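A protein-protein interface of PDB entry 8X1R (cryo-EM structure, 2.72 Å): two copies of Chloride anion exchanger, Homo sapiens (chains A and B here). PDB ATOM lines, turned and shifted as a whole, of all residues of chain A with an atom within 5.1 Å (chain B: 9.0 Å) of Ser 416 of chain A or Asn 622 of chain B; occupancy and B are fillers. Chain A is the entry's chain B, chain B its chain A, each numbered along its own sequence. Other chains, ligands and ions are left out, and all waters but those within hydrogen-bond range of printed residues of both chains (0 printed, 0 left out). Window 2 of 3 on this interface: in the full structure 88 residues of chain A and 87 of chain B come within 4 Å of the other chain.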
ATOM      1  N   LYS A 294       0.419 -27.080 -23.407  1.00  0.00           N
ATOM      2  CA  LYS A 294      -0.121 -25.742 -23.200  1.00  0.00           C
ATOM      3  C   LYS A 294       0.356 -24.728 -24.233  1.00  0.00           C
ATOM      4  O   LYS A 294      -0.199 -23.627 -24.294  1.00  0.00           O
ATOM      5  CB  LYS A 294       0.248 -25.257 -21.798  1.00  0.00           C
ATOM      6  CG  LYS A 294      -0.744 -24.300 -21.179  1.00  0.00           C
ATOM      7  CD  LYS A 294      -0.372 -23.983 -19.742  1.00  0.00           C
ATOM      8  CE  LYS A 294      -1.503 -23.264 -19.025  1.00  0.00           C
ATOM      9  NZ  LYS A 294      -1.152 -22.916 -17.622  1.00  0.00           N
ATOM     10  N   PRO A 300      -7.341 -24.243 -24.725  1.00  0.00           N
ATOM     11  CA  PRO A 300      -7.408 -25.573 -24.107  1.00  0.00           C
ATOM     12  C   PRO A 300      -8.667 -26.316 -24.528  1.00  0.00           C
ATOM     13  O   PRO A 300      -9.736 -25.726 -24.684  1.00  0.00           O
ATOM     14  CB  PRO A 300      -7.407 -25.272 -22.604  1.00  0.00           C
ATOM     15  CG  PRO A 300      -7.745 -23.825 -22.487  1.00  0.00           C
ATOM     16  CD  PRO A 300      -7.224 -23.174 -23.722  1.00  0.00           C
ATOM     17  N   LYS A 375       0.385 -12.818 -10.071  1.00  0.00           N
ATOM     18  CA  LYS A 375       0.783 -13.145 -11.437  1.00  0.00           C
ATOM     19  C   LYS A 375       0.621 -11.956 -12.376  1.00  0.00           C
ATOM     20  O   LYS A 375       1.420 -11.781 -13.303  1.00  0.00           O
ATOM     21  CB  LYS A 375      -0.021 -14.339 -11.944  1.00  0.00           C
ATOM     22  CG  LYS A 375       0.324 -14.770 -13.356  1.00  0.00           C
ATOM     23  CD  LYS A 375      -0.339 -16.085 -13.697  1.00  0.00           C
ATOM     24  CE  LYS A 375       0.163 -16.631 -15.015  1.00  0.00           C
ATOM     25  NZ  LYS A 375      -0.686 -16.215 -16.156  1.00  0.00           N
ATOM     26  N   SER A 411     -11.484 -21.066 -11.937  1.00  0.00           N
ATOM     27  CA  SER A 411     -10.644 -19.881 -12.082  1.00  0.00           C
ATOM     28  C   SER A 411      -9.497 -20.144 -13.047  1.00  0.00           C
ATOM     29  O   SER A 411      -9.103 -19.253 -13.806  1.00  0.00           O
ATOM     30  CB  SER A 411     -10.102 -19.447 -10.727  1.00  0.00           C
ATOM     31  OG  SER A 411     -11.027 -19.746  -9.711  1.00  0.00           O
ATOM     32  N   ALA A 412      -8.957 -21.363 -13.037  1.00  0.00           N
ATOM     33  CA  ALA A 412      -7.915 -21.714 -13.992  1.00  0.00           C
ATOM     34  C   ALA A 412      -8.465 -21.784 -15.408  1.00  0.00           C
ATOM     35  O   ALA A 412      -7.787 -21.391 -16.359  1.00  0.00           O
ATOM     36  CB  ALA A 412      -7.272 -23.040 -13.600  1.00  0.00           C
ATOM     37  N   VAL A 413      -9.686 -22.297 -15.573  1.00  0.00           N
ATOM     38  CA  VAL A 413     -10.300 -22.322 -16.900  1.00  0.00           C
ATOM     39  C   VAL A 413     -10.568 -20.904 -17.393  1.00  0.00           C
ATOM     40  O   VAL A 413     -10.504 -20.624 -18.595  1.00  0.00           O
ATOM     41  CB  VAL A 413     -11.584 -23.171 -16.890  1.00  0.00           C
ATOM     42  CG1 VAL A 413     -12.179 -23.241 -18.276  1.00  0.00           C
ATOM     43  CG2 VAL A 413     -11.277 -24.571 -16.422  1.00  0.00           C
ATOM     44  N   GLN A 414     -10.876 -19.987 -16.474  1.00  0.00           N
ATOM     45  CA  GLN A 414     -11.151 -18.614 -16.883  1.00  0.00           C
ATOM     46  C   GLN A 414      -9.871 -17.870 -17.229  1.00  0.00           C
ATOM     47  O   GLN A 414      -9.833 -17.106 -18.197  1.00  0.00           O
ATOM     48  CB  GLN A 414     -11.910 -17.866 -15.791  1.00  0.00           C
ATOM     49  CG  GLN A 414     -12.509 -16.565 -16.285  1.00  0.00           C
ATOM     50  CD  GLN A 414     -13.075 -15.709 -15.181  1.00  0.00           C
ATOM     51  OE1 GLN A 414     -13.729 -16.206 -14.272  1.00  0.00           O
ATOM     52  NE2 GLN A 414     -12.832 -14.410 -15.259  1.00  0.00           N
ATOM     53  N   GLU A 415      -8.813 -18.072 -16.445  1.00  0.00           N
ATOM     54  CA  GLU A 415      -7.565 -17.356 -16.679  1.00  0.00           C
ATOM     55  C   GLU A 415      -6.801 -17.932 -17.863  1.00  0.00           C
ATOM     56  O   GLU A 415      -6.208 -17.182 -18.645  1.00  0.00           O
ATOM     57  CB  GLU A 415      -6.703 -17.391 -15.420  1.00  0.00           C
ATOM     58  CG  GLU A 415      -5.363 -16.695 -15.560  1.00  0.00           C
ATOM     59  CD  GLU A 415      -4.211 -17.661 -15.770  1.00  0.00           C
ATOM     60  OE1 GLU A 415      -4.309 -18.824 -15.326  1.00  0.00           O
ATOM     61  OE2 GLU A 415      -3.202 -17.254 -16.380  1.00  0.00           O
ATOM     62  N   SER A 416      -6.804 -19.253 -18.011  1.00  0.00           N
ATOM     63  CA  SER A 416      -6.085 -19.927 -19.079  1.00  0.00           C
ATOM     64  C   SER A 416      -6.674 -19.669 -20.456  1.00  0.00           C
ATOM     65  O   SER A 416      -5.970 -19.851 -21.453  1.00  0.00           O
ATOM     66  CB  SER A 416      -6.062 -21.431 -18.812  1.00  0.00           C
ATOM     67  OG  SER A 416      -5.871 -22.153 -20.014  1.00  0.00           O
ATOM     68  N   THR A 417      -7.933 -19.254 -20.536  1.00  0.00           N
ATOM     69  CA  THR A 417      -8.598 -19.032 -21.809  1.00  0.00           C
ATOM     70  C   THR A 417      -8.554 -17.574 -22.243  1.00  0.00           C
ATOM     71  O   THR A 417      -9.132 -17.225 -23.275  1.00  0.00           O
ATOM     72  CB  THR A 417     -10.048 -19.511 -21.726  1.00  0.00           C
ATOM     73  OG1 THR A 417     -10.123 -20.641 -20.850  1.00  0.00           O
ATOM     74  CG2 THR A 417     -10.534 -19.947 -23.090  1.00  0.00           C
ATOM     75  N   GLY A 418      -7.877 -16.719 -21.486  1.00  0.00           N
ATOM     76  CA  GLY A 418      -7.728 -15.327 -21.845  1.00  0.00           C
ATOM     77  C   GLY A 418      -8.467 -14.349 -20.967  1.00  0.00           C
ATOM     78  O   GLY A 418      -8.605 -13.186 -21.356  1.00  0.00           O
ATOM     79  N   GLU B 618       1.896  -6.667 -25.272  1.00  0.00           N
ATOM     80  CA  GLU B 618       0.635  -7.159 -24.721  1.00  0.00           C
ATOM     81  C   GLU B 618       0.639  -8.690 -24.671  1.00  0.00           C
ATOM     82  O   GLU B 618      -0.080  -9.381 -25.392  1.00  0.00           O
ATOM     83  CB  GLU B 618      -0.556  -6.608 -25.516  1.00  0.00           C
ATOM     84  CG  GLU B 618      -1.929  -6.955 -24.946  1.00  0.00           C
ATOM     85  CD  GLU B 618      -2.738  -7.854 -25.860  1.00  0.00           C
ATOM     86  OE1 GLU B 618      -2.809  -7.560 -27.072  1.00  0.00           O
ATOM     87  OE2 GLU B 618      -3.308  -8.851 -25.368  1.00  0.00           O
ATOM     88  N   LEU B 619       1.521  -9.199 -23.816  1.00  0.00           N
ATOM     89  CA  LEU B 619       1.651 -10.635 -23.626  1.00  0.00           C
ATOM     90  C   LEU B 619       0.360 -11.216 -23.062  1.00  0.00           C
ATOM     91  O   LEU B 619      -0.364 -10.562 -22.308  1.00  0.00           O
ATOM     92  CB  LEU B 619       2.818 -10.943 -22.688  1.00  0.00           C
ATOM     93  CG  LEU B 619       4.224 -10.866 -23.277  1.00  0.00           C
ATOM     94  CD1 LEU B 619       4.736  -9.438 -23.272  1.00  0.00           C
ATOM     95  CD2 LEU B 619       5.164 -11.766 -22.506  1.00  0.00           C
ATOM     96  N   ASP B 620       0.072 -12.456 -23.436  1.00  0.00           N
ATOM     97  CA  ASP B 620      -1.163 -13.092 -23.012  1.00  0.00           C
ATOM     98  C   ASP B 620      -0.970 -13.827 -21.689  1.00  0.00           C
ATOM     99  O   ASP B 620       0.108 -13.818 -21.094  1.00  0.00           O
ATOM    100  CB  ASP B 620      -1.676 -14.052 -24.083  1.00  0.00           C
ATOM    101  CG  ASP B 620      -0.708 -15.170 -24.372  1.00  0.00           C
ATOM    102  OD1 ASP B 620       0.460 -14.871 -24.691  1.00  0.00           O
ATOM    103  OD2 ASP B 620      -1.115 -16.347 -24.288  1.00  0.00           O
ATOM    104  N   ASN B 621      -2.047 -14.465 -21.234  1.00  0.00           N
ATOM    105  CA  ASN B 621      -2.068 -15.049 -19.900  1.00  0.00           C
ATOM    106  C   ASN B 621      -1.128 -16.234 -19.760  1.00  0.00           C
ATOM    107  O   ASN B 621      -0.709 -16.550 -18.642  1.00  0.00           O
ATOM    108  CB  ASN B 621      -3.493 -15.477 -19.546  1.00  0.00           C
ATOM    109  CG  ASN B 621      -4.437 -14.303 -19.416  1.00  0.00           C
ATOM    110  OD1 ASN B 621      -4.336 -13.326 -20.155  1.00  0.00           O
ATOM    111  ND2 ASN B 621      -5.361 -14.390 -18.473  1.00  0.00           N
ATOM    112  N   ASN B 622      -0.788 -16.900 -20.859  1.00  0.00           N
ATOM    113  CA  ASN B 622       0.063 -18.079 -20.817  1.00  0.00           C
ATOM    114  C   ASN B 622       1.500 -17.785 -21.213  1.00  0.00           C
ATOM    115  O   ASN B 622       2.331 -18.698 -21.203  1.00  0.00           O
ATOM    116  CB  ASN B 622      -0.510 -19.175 -21.720  1.00  0.00           C
ATOM    117  CG  ASN B 622      -1.931 -19.543 -21.352  1.00  0.00           C
ATOM    118  OD1 ASN B 622      -2.791 -19.691 -22.219  1.00  0.00           O
ATOM    119  ND2 ASN B 622      -2.189 -19.691 -20.058  1.00  0.00           N
ATOM    120  N   GLN B 623       1.815 -16.539 -21.557  1.00  0.00           N
ATOM    121  CA  GLN B 623       3.169 -16.153 -21.917  1.00  0.00           C
ATOM    122  C   GLN B 623       3.738 -15.070 -21.019  1.00  0.00           C
ATOM    123  O   GLN B 623       4.882 -14.660 -21.229  1.00  0.00           O
ATOM    124  CB  GLN B 623       3.219 -15.660 -23.370  1.00  0.00           C
ATOM    125  CG  GLN B 623       3.641 -16.709 -24.375  1.00  0.00           C
ATOM    126  CD  GLN B 623       3.318 -16.304 -25.798  1.00  0.00           C
ATOM    127  OE1 GLN B 623       3.601 -17.038 -26.745  1.00  0.00           O
ATOM    128  NE2 GLN B 623       2.721 -15.127 -25.958  1.00  0.00           N
ATOM    129  N   ILE B 624       2.983 -14.598 -20.026  1.00  0.00           N
ATOM    130  CA  ILE B 624       3.411 -13.428 -19.272  1.00  0.00           C
ATOM    131  C   ILE B 624       4.398 -13.788 -18.171  1.00  0.00           C
ATOM    132  O   ILE B 624       5.225 -12.950 -17.789  1.00  0.00           O
ATOM    133  CB  ILE B 624       2.181 -12.683 -18.719  1.00  0.00           C
ATOM    134  CG1 ILE B 624       2.487 -11.195 -18.567  1.00  0.00           C
ATOM    135  CG2 ILE B 624       1.719 -13.280 -17.404  1.00  0.00           C
ATOM    136  CD1 ILE B 624       1.290 -10.365 -18.188  1.00  0.00           C
ATOM    137  N   GLU B 625       4.371 -15.025 -17.673  1.00  0.00           N
ATOM    138  CA  GLU B 625       5.319 -15.409 -16.634  1.00  0.00           C
ATOM    139  C   GLU B 625       6.749 -15.464 -17.140  1.00  0.00           C
ATOM    140  O   GLU B 625       7.656 -15.731 -16.348  1.00  0.00           O
ATOM    141  CB  GLU B 625       4.931 -16.758 -16.027  1.00  0.00           C
ATOM    142  CG  GLU B 625       3.778 -16.738 -15.009  1.00  0.00           C
ATOM    143  CD  GLU B 625       4.008 -15.845 -13.784  1.00  0.00           C
ATOM    144  OE1 GLU B 625       4.303 -14.639 -13.929  1.00  0.00           O
ATOM    145  OE2 GLU B 625       3.883 -16.363 -12.654  1.00  0.00           O
ATOM    146  N   VAL B 626       6.973 -15.222 -18.435  1.00  0.00           N
ATOM    147  CA  VAL B 626       8.327 -15.056 -18.952  1.00  0.00           C
ATOM    148  C   VAL B 626       8.955 -13.750 -18.504  1.00  0.00           C
ATOM    149  O   VAL B 626      10.167 -13.568 -18.673  1.00  0.00           O
ATOM    150  CB  VAL B 626       8.334 -15.138 -20.491  1.00  0.00           C
ATOM    151  CG1 VAL B 626       8.038 -13.781 -21.101  1.00  0.00           C
ATOM    152  CG2 VAL B 626       9.660 -15.676 -20.991  1.00  0.00           C
ATOM    153  N   LEU B 627       8.172 -12.834 -17.931  1.00  0.00           N
ATOM    154  CA  LEU B 627       8.733 -11.589 -17.428  1.00  0.00           C
ATOM    155  C   LEU B 627       9.382 -11.739 -16.060  1.00  0.00           C
ATOM    156  O   LEU B 627      10.045 -10.803 -15.605  1.00  0.00           O
ATOM    157  CB  LEU B 627       7.651 -10.510 -17.358  1.00  0.00           C
ATOM    158  CG  LEU B 627       6.981 -10.117 -18.671  1.00  0.00           C
ATOM    159  CD1 LEU B 627       6.130  -8.883 -18.476  1.00  0.00           C
ATOM    160  CD2 LEU B 627       8.009  -9.888 -19.755  1.00  0.00           C
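The side-chain amino group (NZ) of Lys 375 of chain A sits at hydrogen-bond distance from the backbone carbonyl oxygen (O) of Asn 621 of chain B, 2.5 Å away. ND2 of Asn 621 of chain B sits at hydrogen-bond distance from O of Glu 415 of chain A (2.9 Å). The backbone carbonyl oxygen of Ser 416 of chain A sits close to the side-chain amide oxygen of Asn 622 of chain B.
NZ of Lys 375 of chain A lies within salt-bridge range of OE2 of Glu 415 of chain A (2.7 Å). OD2 of Asp 620 of chain B lies close to N of Asn 622 of chain B, at 3.5 Å.
Lys 294 of chain A touches Asn 622 of chain B (CE to ND2, 3.8 Å). CG2 of Ile 624 of chain B touches NZ of Lys 375 of chain A, 3.99 Å away. Lys 375 of chain A touches Glu 625 of chain B (CE to CG, 3.6 Å). C of Gly 418 of chain A touches ND2 of Asn 621 of chain B (3.98 Å).
No residue of chain B comes within 4 Å of Thr 417 of chain A. Of the printed residues of chain B, Gly 418 of chain A touches Asn 621. Printed residues of chain A within 4 Å of Ile 624 of chain B: Lys 375. Of the printed residues of chain B, Lys 294 of chain A touches Asn 622. Printed residues of chain B within 4 Å of Lys 375 of chain A: Asn 621 (2.5 Å), Ile 624 (3.99 Å) and Glu 625 (3.6 Å). Of the printed residues of chain A, Glu 625 of chain B touches Lys 375 (3.6 Å). The nearest residue of chain B that does not touch Ser 416 of chain A is Asn 621 of chain B (5.1 Å). The nearest residue of chain A that does not touch Asn 622 of chain B is Glu 415 of chain A (4.5 Å). The nearest printed residue of chain A that does not touch Glu 625 of chain B is Glu 415 of chain A (7.1 Å).
Printed residues of chain B that touch a printed residue of chain A: Asn 621, Asn 622, Ile 624 and Glu 625. Along chain B the printed residues that touch a printed residue of chain A span positions 621 to 625. Printed residues of chain A that touch a printed residue of chain B: Lys 294, Lys 375, Glu 415, Ser 416 and Gly 418. Along chain A the printed residues that touch a printed residue of chain B span positions 294 to 418. Among the printed residues, no Asp or Glu carboxylate lies within 4 Å of a Lys or Arg side-chain nitrogen of the other chain.
No position is printed for both chains.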
